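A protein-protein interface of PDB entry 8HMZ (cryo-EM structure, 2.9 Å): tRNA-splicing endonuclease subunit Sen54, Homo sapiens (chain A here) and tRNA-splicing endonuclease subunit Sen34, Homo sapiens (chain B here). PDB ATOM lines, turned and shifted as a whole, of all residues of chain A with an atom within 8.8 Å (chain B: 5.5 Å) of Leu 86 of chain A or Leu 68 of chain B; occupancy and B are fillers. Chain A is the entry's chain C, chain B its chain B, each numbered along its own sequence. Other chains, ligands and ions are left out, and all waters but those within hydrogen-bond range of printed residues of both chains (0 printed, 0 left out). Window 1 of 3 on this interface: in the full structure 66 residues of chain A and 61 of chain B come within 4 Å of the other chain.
The side-chain hydroxyl (OG1) of Thr 209 of chain B is in hydrogen-bond range of the side-chain amide nitrogen (NE2) of Gln 89 of chain A, at 2.6 Å.
The backbone carbonyl oxygen of Thr 209 of chain B is in hydrogen-bond range of the backbone NH of Gln 158 of chain A (3.1 Å).
O of Gly 67 of chain B lies within hydrogen-bond range of N of Gly 54 of chain B (3.0 Å).
The backbone carbonyl oxygen (O) of Arg 36 of chain A lies close to the side-chain amide oxygen (OE1) of Gln 89 of chain A (3.5 Å).
The backbone carbonyl oxygen of Gln 89 of chain A is in hydrogen-bond range of the guanidinium group of Arg 49 of chain A, at 3.3 Å.
NE of Arg 90 of chain A is in hydrogen-bond range of O of Glu 142 of chain A (2.6 Å).
OE1 of Glu 142 of chain A lies within hydrogen-bond range of OH of Tyr 161 of chain A (3.3 Å).
Among the printed residues, pairs that only touch across the chains: Leu 86 of chain A with Gly 67 of chain B (3.8 Å), Leu 86 of chain A with Leu 68 of chain B (3.6 Å), Arg 90 of chain A with Ala 55 of chain B (3.7 Å), Glu 142 of chain A with Ala 55 of chain B (3.9 Å), Ile 157 of chain A with Trp 34 of chain B (3.9 Å), Ile 157 of chain A with Thr 209 of chain B (3.8 Å), Gln 158 of chain A with Trp 34 of chain B (3.6 Å), Tyr 161 of chain A with Trp 34 of chain B (3.7 Å), Arg 183 of chain A with Gly 54 of chain B (3.8 Å) and Arg 183 of chain A with Leu 66 of chain B (3.997 Å).
Leu 86 of chain A touches just these residues of chain B: Gly 67 (3.8 Å) and Leu 68 (3.6 Å).
Leu 68 of chain B touches one residue of chain A.
No residue of chain A comes within 4 Å of Gly 35 of chain B.
No residue of chain A comes within 4 Å of Pro 69 of chain B.
Of the printed residues of chain B, Gln 158 of chain A touches Trp 34 and Thr 209.
Of the printed residues of chain A, Gly 54 of chain B touches Arg 183 (3.8 Å).
Printed residues of chain A within 4 Å of Trp 34 of chain B: Ile 157 (3.9 Å), Gln 158 (3.6 Å) and Tyr 161 (3.7 Å).
Of the printed residues of chain A, Leu 66 of chain B touches Arg 183 (3.997 Å).
Of the printed residues of chain B, Gln 89 of chain A touches Thr 209.
Ala 36 of chain B touches none of the printed residues of chain A.
The nearest printed residue of chain B that does not touch Leu 86 of chain A is Ala 36 of chain B (4.1 Å).
The nearest residue of chain A that does not touch Leu 68 of chain B is Glu 142 of chain A (5.1 Å).
Printed residues of chain B that touch a printed residue of chain A: Trp 34, Gly 54, Ala 55, Leu 66, Gly 67, Leu 68 and Thr 209.
Hydrophobic or aromatic side chains of chain B that line the printed part of chain A: Trp 34, Ala 55, Leu 66 and Leu 68.
Hydrophobic or aromatic side chains of chain A that line the printed part of chain B: Leu 86, Ile 157 and Tyr 161.
Among the printed residues, no Asp or Glu carboxylate lies within 4 Å of a Lys or Arg side-chain nitrogen of the other chain.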
ATOM      1  N   ARG A  36      27.693  17.350 -13.849  1.00  0.00           N
ATOM      2  CA  ARG A  36      27.066  16.318 -14.667  1.00  0.00           C
ATOM      3  C   ARG A  36      25.980  16.981 -15.502  1.00  0.00           C
ATOM      4  O   ARG A  36      25.065  17.600 -14.950  1.00  0.00           O
ATOM      5  CB  ARG A  36      26.472  15.213 -13.793  1.00  0.00           C
ATOM      6  CG  ARG A  36      25.470  14.318 -14.505  1.00  0.00           C
ATOM      7  CD  ARG A  36      24.878  13.296 -13.550  1.00  0.00           C
ATOM      8  NE  ARG A  36      24.849  13.796 -12.177  1.00  0.00           N
ATOM      9  CZ  ARG A  36      23.792  13.721 -11.376  1.00  0.00           C
ATOM     10  NH1 ARG A  36      23.857  14.206 -10.143  1.00  0.00           N
ATOM     11  NH2 ARG A  36      22.669  13.159 -11.804  1.00  0.00           N
ATOM     12  N   ARG A  49       8.935  12.448 -13.315  1.00  0.00           N
ATOM     13  CA  ARG A  49       9.378  11.938 -12.027  1.00  0.00           C
ATOM     14  C   ARG A  49       8.189  11.755 -11.093  1.00  0.00           C
ATOM     15  O   ARG A  49       7.144  12.389 -11.256  1.00  0.00           O
ATOM     16  CB  ARG A  49      10.402  12.889 -11.404  1.00  0.00           C
ATOM     17  CG  ARG A  49      11.186  12.311 -10.237  1.00  0.00           C
ATOM     18  CD  ARG A  49      12.249  13.284  -9.757  1.00  0.00           C
ATOM     19  NE  ARG A  49      13.448  13.211 -10.586  1.00  0.00           N
ATOM     20  CZ  ARG A  49      14.307  14.212 -10.757  1.00  0.00           C
ATOM     21  NH1 ARG A  49      14.110  15.374 -10.151  1.00  0.00           N
ATOM     22  NH2 ARG A  49      15.367  14.046 -11.535  1.00  0.00           N
ATOM     23  N   PRO A  54      11.389   7.816  -0.696  1.00  0.00           N
ATOM     24  CA  PRO A  54      11.684   6.489  -0.154  1.00  0.00           C
ATOM     25  C   PRO A  54      11.663   6.518   1.364  1.00  0.00           C
ATOM     26  O   PRO A  54      11.895   7.550   1.998  1.00  0.00           O
ATOM     27  CB  PRO A  54      13.091   6.185  -0.681  1.00  0.00           C
ATOM     28  CG  PRO A  54      13.312   7.152  -1.800  1.00  0.00           C
ATOM     29  CD  PRO A  54      12.524   8.372  -1.447  1.00  0.00           C
ATOM     30  N   ARG A  79      21.205   1.591   1.271  1.00  0.00           N
ATOM     31  CA  ARG A  79      22.195   2.475   0.668  1.00  0.00           C
ATOM     32  C   ARG A  79      21.912   2.762  -0.800  1.00  0.00           C
ATOM     33  O   ARG A  79      21.917   3.925  -1.208  1.00  0.00           O
ATOM     34  CB  ARG A  79      23.600   1.884   0.807  1.00  0.00           C
ATOM     35  CG  ARG A  79      24.310   2.261   2.085  1.00  0.00           C
ATOM     36  CD  ARG A  79      25.566   1.441   2.247  1.00  0.00           C
ATOM     37  NE  ARG A  79      26.398   1.926   3.340  1.00  0.00           N
ATOM     38  CZ  ARG A  79      27.491   1.309   3.769  1.00  0.00           C
ATOM     39  NH1 ARG A  79      27.888   0.187   3.189  1.00  0.00           N
ATOM     40  NH2 ARG A  79      28.191   1.816   4.772  1.00  0.00           N
ATOM     41  N   GLU A  80      21.676   1.723  -1.607  1.00  0.00           N
ATOM     42  CA  GLU A  80      21.390   1.930  -3.025  1.00  0.00           C
ATOM     43  C   GLU A  80      20.207   2.862  -3.255  1.00  0.00           C
ATOM     44  O   GLU A  80      20.081   3.430  -4.344  1.00  0.00           O
ATOM     45  CB  GLU A  80      21.135   0.594  -3.721  1.00  0.00           C
ATOM     46  CG  GLU A  80      22.254  -0.416  -3.556  1.00  0.00           C
ATOM     47  CD  GLU A  80      23.303  -0.314  -4.645  1.00  0.00           C
ATOM     48  OE1 GLU A  80      23.194   0.595  -5.495  1.00  0.00           O
ATOM     49  OE2 GLU A  80      24.236  -1.143  -4.652  1.00  0.00           O
ATOM     50  N   GLU A  81      19.338   3.031  -2.258  1.00  0.00           N
ATOM     51  CA  GLU A  81      18.258   4.003  -2.357  1.00  0.00           C
ATOM     52  C   GLU A  81      18.738   5.419  -2.074  1.00  0.00           C
ATOM     53  O   GLU A  81      18.143   6.380  -2.568  1.00  0.00           O
ATOM     54  CB  GLU A  81      17.133   3.639  -1.391  1.00  0.00           C
ATOM     55  CG  GLU A  81      16.051   2.765  -1.989  1.00  0.00           C
ATOM     56  CD  GLU A  81      14.823   2.694  -1.109  1.00  0.00           C
ATOM     57  OE1 GLU A  81      13.707   2.925  -1.620  1.00  0.00           O
ATOM     58  OE2 GLU A  81      14.975   2.417   0.099  1.00  0.00           O
ATOM     59  N   LEU A  82      19.789   5.567  -1.267  1.00  0.00           N
ATOM     60  CA  LEU A  82      20.312   6.894  -0.965  1.00  0.00           C
ATOM     61  C   LEU A  82      21.069   7.474  -2.153  1.00  0.00           C
ATOM     62  O   LEU A  82      20.922   8.656  -2.478  1.00  0.00           O
ATOM     63  CB  LEU A  82      21.203   6.833   0.274  1.00  0.00           C
ATOM     64  CG  LEU A  82      21.607   8.184   0.853  1.00  0.00           C
ATOM     65  CD1 LEU A  82      20.402   8.871   1.449  1.00  0.00           C
ATOM     66  CD2 LEU A  82      22.676   7.997   1.906  1.00  0.00           C
ATOM     67  N   TRP A  83      21.893   6.659  -2.812  1.00  0.00           N
ATOM     68  CA  TRP A  83      22.673   7.140  -3.946  1.00  0.00           C
ATOM     69  C   TRP A  83      21.823   7.423  -5.173  1.00  0.00           C
ATOM     70  O   TRP A  83      22.343   7.986  -6.142  1.00  0.00           O
ATOM     71  CB  TRP A  83      23.765   6.130  -4.300  1.00  0.00           C
ATOM     72  CG  TRP A  83      24.488   5.529  -3.126  1.00  0.00           C
ATOM     73  CD1 TRP A  83      24.882   4.233  -2.997  1.00  0.00           C
ATOM     74  CD2 TRP A  83      24.934   6.200  -1.936  1.00  0.00           C
ATOM     75  NE1 TRP A  83      25.527   4.047  -1.801  1.00  0.00           N
ATOM     76  CE2 TRP A  83      25.571   5.240  -1.131  1.00  0.00           C
ATOM     77  CE3 TRP A  83      24.847   7.516  -1.470  1.00  0.00           C
ATOM     78  CZ2 TRP A  83      26.117   5.551   0.108  1.00  0.00           C
ATOM     79  CZ3 TRP A  83      25.387   7.819  -0.240  1.00  0.00           C
ATOM     80  CH2 TRP A  83      26.012   6.842   0.536  1.00  0.00           C
ATOM     81  N   GLN A  84      20.544   7.050  -5.164  1.00  0.00           N
ATOM     82  CA  GLN A  84      19.626   7.417  -6.233  1.00  0.00           C
ATOM     83  C   GLN A  84      18.946   8.749  -5.957  1.00  0.00           C
ATOM     84  O   GLN A  84      18.697   9.522  -6.886  1.00  0.00           O
ATOM     85  CB  GLN A  84      18.568   6.330  -6.414  1.00  0.00           C
ATOM     86  CG  GLN A  84      19.037   5.111  -7.181  1.00  0.00           C
ATOM     87  CD  GLN A  84      17.890   4.189  -7.541  1.00  0.00           C
ATOM     88  OE1 GLN A  84      16.740   4.617  -7.625  1.00  0.00           O
ATOM     89  NE2 GLN A  84      18.196   2.913  -7.739  1.00  0.00           N
ATOM     90  N   LEU A  85      18.638   9.024  -4.691  1.00  0.00           N
ATOM     91  CA  LEU A  85      18.010  10.289  -4.330  1.00  0.00           C
ATOM     92  C   LEU A  85      18.961  11.459  -4.542  1.00  0.00           C
ATOM     93  O   LEU A  85      18.587  12.480  -5.131  1.00  0.00           O
ATOM     94  CB  LEU A  85      17.535  10.233  -2.880  1.00  0.00           C
ATOM     95  CG  LEU A  85      16.263  11.011  -2.560  1.00  0.00           C
ATOM     96  CD1 LEU A  85      15.104  10.502  -3.400  1.00  0.00           C
ATOM     97  CD2 LEU A  85      15.943  10.919  -1.083  1.00  0.00           C
ATOM     98  N   LEU A  86      20.197  11.336  -4.054  1.00  0.00           N
ATOM     99  CA  LEU A  86      21.143  12.444  -4.141  1.00  0.00           C
ATOM    100  C   LEU A  86      21.625  12.700  -5.562  1.00  0.00           C
ATOM    101  O   LEU A  86      22.127  13.793  -5.840  1.00  0.00           O
ATOM    102  CB  LEU A  86      22.343  12.189  -3.231  1.00  0.00           C
ATOM    103  CG  LEU A  86      22.039  11.890  -1.765  1.00  0.00           C
ATOM    104  CD1 LEU A  86      23.321  11.591  -1.018  1.00  0.00           C
ATOM    105  CD2 LEU A  86      21.300  13.047  -1.122  1.00  0.00           C
ATOM    106  N   ALA A  87      21.496  11.730  -6.459  1.00  0.00           N
ATOM    107  CA  ALA A  87      21.888  11.914  -7.854  1.00  0.00           C
ATOM    108  C   ALA A  87      20.680  12.308  -8.702  1.00  0.00           C
ATOM    109  O   ALA A  87      20.351  11.680  -9.707  1.00  0.00           O
ATOM    110  CB  ALA A  87      22.548  10.647  -8.387  1.00  0.00           C
ATOM    111  N   GLU A  88      20.021  13.384  -8.278  1.00  0.00           N
ATOM    112  CA  GLU A  88      18.829  13.891  -8.942  1.00  0.00           C
ATOM    113  C   GLU A  88      18.996  15.383  -9.178  1.00  0.00           C
ATOM    114  O   GLU A  88      19.287  16.132  -8.241  1.00  0.00           O
ATOM    115  CB  GLU A  88      17.575  13.627  -8.109  1.00  0.00           C
ATOM    116  CG  GLU A  88      16.957  12.264  -8.341  1.00  0.00           C
ATOM    117  CD  GLU A  88      15.614  12.117  -7.663  1.00  0.00           C
ATOM    118  OE1 GLU A  88      14.873  11.171  -8.005  1.00  0.00           O
ATOM    119  OE2 GLU A  88      15.295  12.951  -6.790  1.00  0.00           O
ATOM    120  N   GLN A  89      18.817  15.805 -10.423  1.00  0.00           N
ATOM    121  CA  GLN A  89      18.950  17.199 -10.809  1.00  0.00           C
ATOM    122  C   GLN A  89      17.579  17.832 -11.001  1.00  0.00           C
ATOM    123  O   GLN A  89      16.601  17.154 -11.320  1.00  0.00           O
ATOM    124  CB  GLN A  89      19.765  17.326 -12.098  1.00  0.00           C
ATOM    125  CG  GLN A  89      21.125  16.645 -12.059  1.00  0.00           C
ATOM    126  CD  GLN A  89      22.194  17.496 -11.404  1.00  0.00           C
ATOM    127  OE1 GLN A  89      23.120  17.960 -12.065  1.00  0.00           O
ATOM    128  NE2 GLN A  89      22.079  17.695 -10.098  1.00  0.00           N
ATOM    129  N   ARG A  90      17.516  19.146 -10.799  1.00  0.00           N
ATOM    130  CA  ARG A  90      16.300  19.894 -11.074  1.00  0.00           C
ATOM    131  C   ARG A  90      16.145  20.104 -12.573  1.00  0.00           C
ATOM    132  O   ARG A  90      17.107  20.429 -13.273  1.00  0.00           O
ATOM    133  CB  ARG A  90      16.321  21.247 -10.365  1.00  0.00           C
ATOM    134  CG  ARG A  90      16.261  21.172  -8.855  1.00  0.00           C
ATOM    135  CD  ARG A  90      16.725  22.478  -8.237  1.00  0.00           C
ATOM    136  NE  ARG A  90      16.690  22.446  -6.779  1.00  0.00           N
ATOM    137  CZ  ARG A  90      17.631  21.898  -6.019  1.00  0.00           C
ATOM    138  NH1 ARG A  90      18.690  21.328  -6.574  1.00  0.00           N
ATOM    139  NH2 ARG A  90      17.514  21.924  -4.701  1.00  0.00           N
ATOM    140  N   GLU A 142      16.531  27.363  -5.248  1.00  0.00           N
ATOM    141  CA  GLU A 142      16.517  25.981  -4.781  1.00  0.00           C
ATOM    142  C   GLU A 142      15.183  25.306  -5.077  1.00  0.00           C
ATOM    143  O   GLU A 142      15.148  24.156  -5.530  1.00  0.00           O
ATOM    144  CB  GLU A 142      16.831  25.923  -3.290  1.00  0.00           C
ATOM    145  CG  GLU A 142      18.312  25.890  -2.984  1.00  0.00           C
ATOM    146  CD  GLU A 142      18.605  25.326  -1.613  1.00  0.00           C
ATOM    147  OE1 GLU A 142      19.439  24.402  -1.515  1.00  0.00           O
ATOM    148  OE2 GLU A 142      18.003  25.807  -0.632  1.00  0.00           O
ATOM    149  N   ILE A 157      23.744  25.905  -8.203  1.00  0.00           N
ATOM    150  CA  ILE A 157      23.499  26.082  -6.779  1.00  0.00           C
ATOM    151  C   ILE A 157      24.794  26.180  -5.979  1.00  0.00           C
ATOM    152  O   ILE A 157      24.826  26.877  -4.957  1.00  0.00           O
ATOM    153  CB  ILE A 157      22.588  24.944  -6.280  1.00  0.00           C
ATOM    154  CG1 ILE A 157      21.180  25.129  -6.853  1.00  0.00           C
ATOM    155  CG2 ILE A 157      22.515  24.912  -4.772  1.00  0.00           C
ATOM    156  CD1 ILE A 157      20.620  23.911  -7.533  1.00  0.00           C
ATOM    157  N   GLN A 158      25.879  25.561  -6.445  1.00  0.00           N
ATOM    158  CA  GLN A 158      27.175  25.755  -5.804  1.00  0.00           C
ATOM    159  C   GLN A 158      27.650  27.196  -5.952  1.00  0.00           C
ATOM    160  O   GLN A 158      28.051  27.839  -4.972  1.00  0.00           O
ATOM    161  CB  GLN A 158      28.199  24.794  -6.402  1.00  0.00           C
ATOM    162  CG  GLN A 158      29.575  24.911  -5.791  1.00  0.00           C
ATOM    163  CD  GLN A 158      30.499  23.808  -6.233  1.00  0.00           C
ATOM    164  OE1 GLN A 158      31.647  23.740  -5.804  1.00  0.00           O
ATOM    165  NE2 GLN A 158      30.012  22.946  -7.111  1.00  0.00           N
ATOM    166  N   TYR A 161      25.469  29.475  -3.874  1.00  0.00           N
ATOM    167  CA  TYR A 161      25.857  29.344  -2.475  1.00  0.00           C
ATOM    168  C   TYR A 161      27.116  30.143  -2.177  1.00  0.00           C
ATOM    169  O   TYR A 161      27.240  30.753  -1.110  1.00  0.00           O
ATOM    170  CB  TYR A 161      26.081  27.870  -2.139  1.00  0.00           C
ATOM    171  CG  TYR A 161      24.938  27.197  -1.420  1.00  0.00           C
ATOM    172  CD1 TYR A 161      25.042  26.854  -0.083  1.00  0.00           C
ATOM    173  CD2 TYR A 161      23.762  26.886  -2.085  1.00  0.00           C
ATOM    174  CE1 TYR A 161      24.005  26.230   0.573  1.00  0.00           C
ATOM    175  CE2 TYR A 161      22.722  26.263  -1.437  1.00  0.00           C
ATOM    176  CZ  TYR A 161      22.847  25.936  -0.110  1.00  0.00           C
ATOM    177  OH  TYR A 161      21.810  25.314   0.539  1.00  0.00           O
ATOM    178  N   ARG A 183      10.086  26.277   4.121  1.00  0.00           N
ATOM    179  CA  ARG A 183       9.610  25.025   3.546  1.00  0.00           C
ATOM    180  C   ARG A 183       8.428  24.431   4.297  1.00  0.00           C
ATOM    181  O   ARG A 183       7.851  23.447   3.826  1.00  0.00           O
ATOM    182  CB  ARG A 183      10.737  23.993   3.492  1.00  0.00           C
ATOM    183  CG  ARG A 183      11.801  24.283   2.458  1.00  0.00           C
ATOM    184  CD  ARG A 183      12.800  23.149   2.383  1.00  0.00           C
ATOM    185  NE  ARG A 183      13.475  22.950   3.660  1.00  0.00           N
ATOM    186  CZ  ARG A 183      14.788  23.043   3.832  1.00  0.00           C
ATOM    187  NH1 ARG A 183      15.571  23.331   2.803  1.00  0.00           N
ATOM    188  NH2 ARG A 183      15.317  22.849   5.031  1.00  0.00           N
ATOM    189  N   VAL B  33      30.565  19.187   0.329  1.00  0.00           N
ATOM    190  CA  VAL B  33      30.745  18.224  -0.749  1.00  0.00           C
ATOM    191  C   VAL B  33      29.542  18.341  -1.672  1.00  0.00           C
ATOM    192  O   VAL B  33      28.395  18.321  -1.210  1.00  0.00           O
ATOM    193  CB  VAL B  33      30.892  16.788  -0.213  1.00  0.00           C
ATOM    194  CG1 VAL B  33      31.090  15.812  -1.354  1.00  0.00           C
ATOM    195  CG2 VAL B  33      32.045  16.706   0.767  1.00  0.00           C
ATOM    196  N   TRP B  34      29.802  18.465  -2.971  1.00  0.00           N
ATOM    197  CA  TRP B  34      28.767  18.788  -3.938  1.00  0.00           C
ATOM    198  C   TRP B  34      28.486  17.686  -4.945  1.00  0.00           C
ATOM    199  O   TRP B  34      27.543  17.824  -5.730  1.00  0.00           O
ATOM    200  CB  TRP B  34      29.138  20.074  -4.693  1.00  0.00           C
ATOM    201  CG  TRP B  34      28.994  21.298  -3.855  1.00  0.00           C
ATOM    202  CD1 TRP B  34      29.982  21.952  -3.187  1.00  0.00           C
ATOM    203  CD2 TRP B  34      27.789  22.022  -3.601  1.00  0.00           C
ATOM    204  NE1 TRP B  34      29.468  23.037  -2.524  1.00  0.00           N
ATOM    205  CE2 TRP B  34      28.122  23.101  -2.763  1.00  0.00           C
ATOM    206  CE3 TRP B  34      26.459  21.862  -3.999  1.00  0.00           C
ATOM    207  CZ2 TRP B  34      27.175  24.016  -2.321  1.00  0.00           C
ATOM    208  CZ3 TRP B  34      25.524  22.768  -3.555  1.00  0.00           C
ATOM    209  CH2 TRP B  34      25.884  23.831  -2.725  1.00  0.00           C
ATOM    210  N   GLY B  35      29.263  16.610  -4.953  1.00  0.00           N
ATOM    211  CA  GLY B  35      29.043  15.513  -5.864  1.00  0.00           C
ATOM    212  C   GLY B  35      28.363  14.339  -5.190  1.00  0.00           C
ATOM    213  O   GLY B  35      28.395  14.194  -3.973  1.00  0.00           O
ATOM    214  N   ALA B  36      27.748  13.488  -6.010  1.00  0.00           N
ATOM    215  CA  ALA B  36      27.028  12.327  -5.508  1.00  0.00           C
ATOM    216  C   ALA B  36      27.892  11.078  -5.419  1.00  0.00           C
ATOM    217  O   ALA B  36      27.546  10.161  -4.667  1.00  0.00           O
ATOM    218  CB  ALA B  36      25.811  12.033  -6.394  1.00  0.00           C
ATOM    219  N   VAL B  39      30.169  11.424  -1.996  1.00  0.00           N
ATOM    220  CA  VAL B  39      29.462  11.023  -0.782  1.00  0.00           C
ATOM    221  C   VAL B  39      29.409   9.505  -0.670  1.00  0.00           C
ATOM    222  O   VAL B  39      29.626   8.938   0.411  1.00  0.00           O
ATOM    223  CB  VAL B  39      28.052  11.637  -0.763  1.00  0.00           C
ATOM    224  CG1 VAL B  39      27.357  11.318   0.542  1.00  0.00           C
ATOM    225  CG2 VAL B  39      28.129  13.134  -0.965  1.00  0.00           C
ATOM    226  N   THR B  52      23.446  15.908   5.068  1.00  0.00           N
ATOM    227  CA  THR B  52      22.867  16.582   3.914  1.00  0.00           C
ATOM    228  C   THR B  52      22.035  17.772   4.372  1.00  0.00           C
ATOM    229  O   THR B  52      21.124  17.624   5.190  1.00  0.00           O
ATOM    230  CB  THR B  52      22.007  15.615   3.105  1.00  0.00           C
ATOM    231  OG1 THR B  52      21.117  14.920   3.983  1.00  0.00           O
ATOM    232  CG2 THR B  52      22.881  14.607   2.383  1.00  0.00           C
ATOM    233  N   VAL B  53      22.344  18.950   3.835  1.00  0.00           N
ATOM    234  CA  VAL B  53      21.742  20.194   4.300  1.00  0.00           C
ATOM    235  C   VAL B  53      20.934  20.905   3.229  1.00  0.00           C
ATOM    236  O   VAL B  53      20.245  21.886   3.547  1.00  0.00           O
ATOM    237  CB  VAL B  53      22.807  21.155   4.871  1.00  0.00           C
ATOM    238  CG1 VAL B  53      23.222  20.716   6.262  1.00  0.00           C
ATOM    239  CG2 VAL B  53      24.012  21.225   3.946  1.00  0.00           C
ATOM    240  N   GLY B  54      20.975  20.453   1.983  1.00  0.00           N
ATOM    241  CA  GLY B  54      20.319  21.147   0.892  1.00  0.00           C
ATOM    242  C   GLY B  54      18.824  20.926   0.878  1.00  0.00           C
ATOM    243  O   GLY B  54      18.180  20.768   1.920  1.00  0.00           O
ATOM    244  N   ALA B  55      18.258  20.932  -0.321  1.00  0.00           N
ATOM    245  CA  ALA B  55      16.848  20.657  -0.532  1.00  0.00           C
ATOM    246  C   ALA B  55      16.700  19.510  -1.520  1.00  0.00           C
ATOM    247  O   ALA B  55      17.632  19.165  -2.251  1.00  0.00           O
ATOM    248  CB  ALA B  55      16.110  21.901  -1.040  1.00  0.00           C
ATOM    249  N   LEU B  66      16.466  15.672   2.880  1.00  0.00           N
ATOM    250  CA  LEU B  66      17.204  16.745   2.235  1.00  0.00           C
ATOM    251  C   LEU B  66      18.286  16.145   1.350  1.00  0.00           C
ATOM    252  O   LEU B  66      18.626  14.965   1.462  1.00  0.00           O
ATOM    253  CB  LEU B  66      17.816  17.700   3.266  1.00  0.00           C
ATOM    254  CG  LEU B  66      16.812  18.407   4.182  1.00  0.00           C
ATOM    255  CD1 LEU B  66      17.518  19.293   5.194  1.00  0.00           C
ATOM    256  CD2 LEU B  66      15.800  19.203   3.377  1.00  0.00           C
ATOM    257  N   GLY B  67      18.827  16.977   0.464  1.00  0.00           N
ATOM    258  CA  GLY B  67      19.811  16.518  -0.495  1.00  0.00           C
ATOM    259  C   GLY B  67      21.121  17.272  -0.431  1.00  0.00           C
ATOM    260  O   GLY B  67      21.460  17.857   0.598  1.00  0.00           O
ATOM    261  N   LEU B  68      21.867  17.261  -1.532  1.00  0.00           N
ATOM    262  CA  LEU B  68      23.171  17.895  -1.573  1.00  0.00           C
ATOM    263  C   LEU B  68      23.037  19.405  -1.392  1.00  0.00           C
ATOM    264  O   LEU B  68      22.002  19.988  -1.720  1.00  0.00           O
ATOM    265  CB  LEU B  68      23.862  17.576  -2.893  1.00  0.00           C
ATOM    266  CG  LEU B  68      24.242  16.111  -3.086  1.00  0.00           C
ATOM    267  CD1 LEU B  68      24.686  15.868  -4.512  1.00  0.00           C
ATOM    268  CD2 LEU B  68      25.317  15.700  -2.105  1.00  0.00           C
ATOM    269  N   PRO B  69      24.081  20.072  -0.872  1.00  0.00           N
ATOM    270  CA  PRO B  69      25.412  19.580  -0.507  1.00  0.00           C
ATOM    271  C   PRO B  69      25.439  18.790   0.791  1.00  0.00           C
ATOM    272  O   PRO B  69      24.474  18.801   1.548  1.00  0.00           O
ATOM    273  CB  PRO B  69      26.212  20.866  -0.353  1.00  0.00           C
ATOM    274  CG  PRO B  69      25.213  21.817   0.171  1.00  0.00           C
ATOM    275  CD  PRO B  69      23.957  21.512  -0.595  1.00  0.00           C
ATOM    276  N   LEU B  70      26.545  18.101   1.038  1.00  0.00           N
ATOM    277  CA  LEU B  70      26.773  17.407   2.294  1.00  0.00           C
ATOM    278  C   LEU B  70      27.798  18.181   3.109  1.00  0.00           C
ATOM    279  O   LEU B  70      28.877  18.512   2.606  1.00  0.00           O
ATOM    280  CB  LEU B  70      27.233  15.969   2.044  1.00  0.00           C
ATOM    281  CG  LEU B  70      27.518  15.107   3.268  1.00  0.00           C
ATOM    282  CD1 LEU B  70      26.927  13.741   3.072  1.00  0.00           C
ATOM    283  CD2 LEU B  70      29.006  14.988   3.476  1.00  0.00           C
ATOM    284  N   THR B 209      23.337  21.306  -9.736  1.00  0.00           N
ATOM    285  CA  THR B 209      23.647  21.339  -8.313  1.00  0.00           C
ATOM    286  C   THR B 209      25.096  21.737  -8.075  1.00  0.00           C
ATOM    287  O   THR B 209      25.386  22.544  -7.186  1.00  0.00           O
ATOM    288  CB  THR B 209      23.364  19.978  -7.678  1.00  0.00           C
ATOM    289  OG1 THR B 209      22.125  19.464  -8.180  1.00  0.00           O
ATOM    290  CG2 THR B 209      23.274  20.102  -6.167  1.00  0.00           C
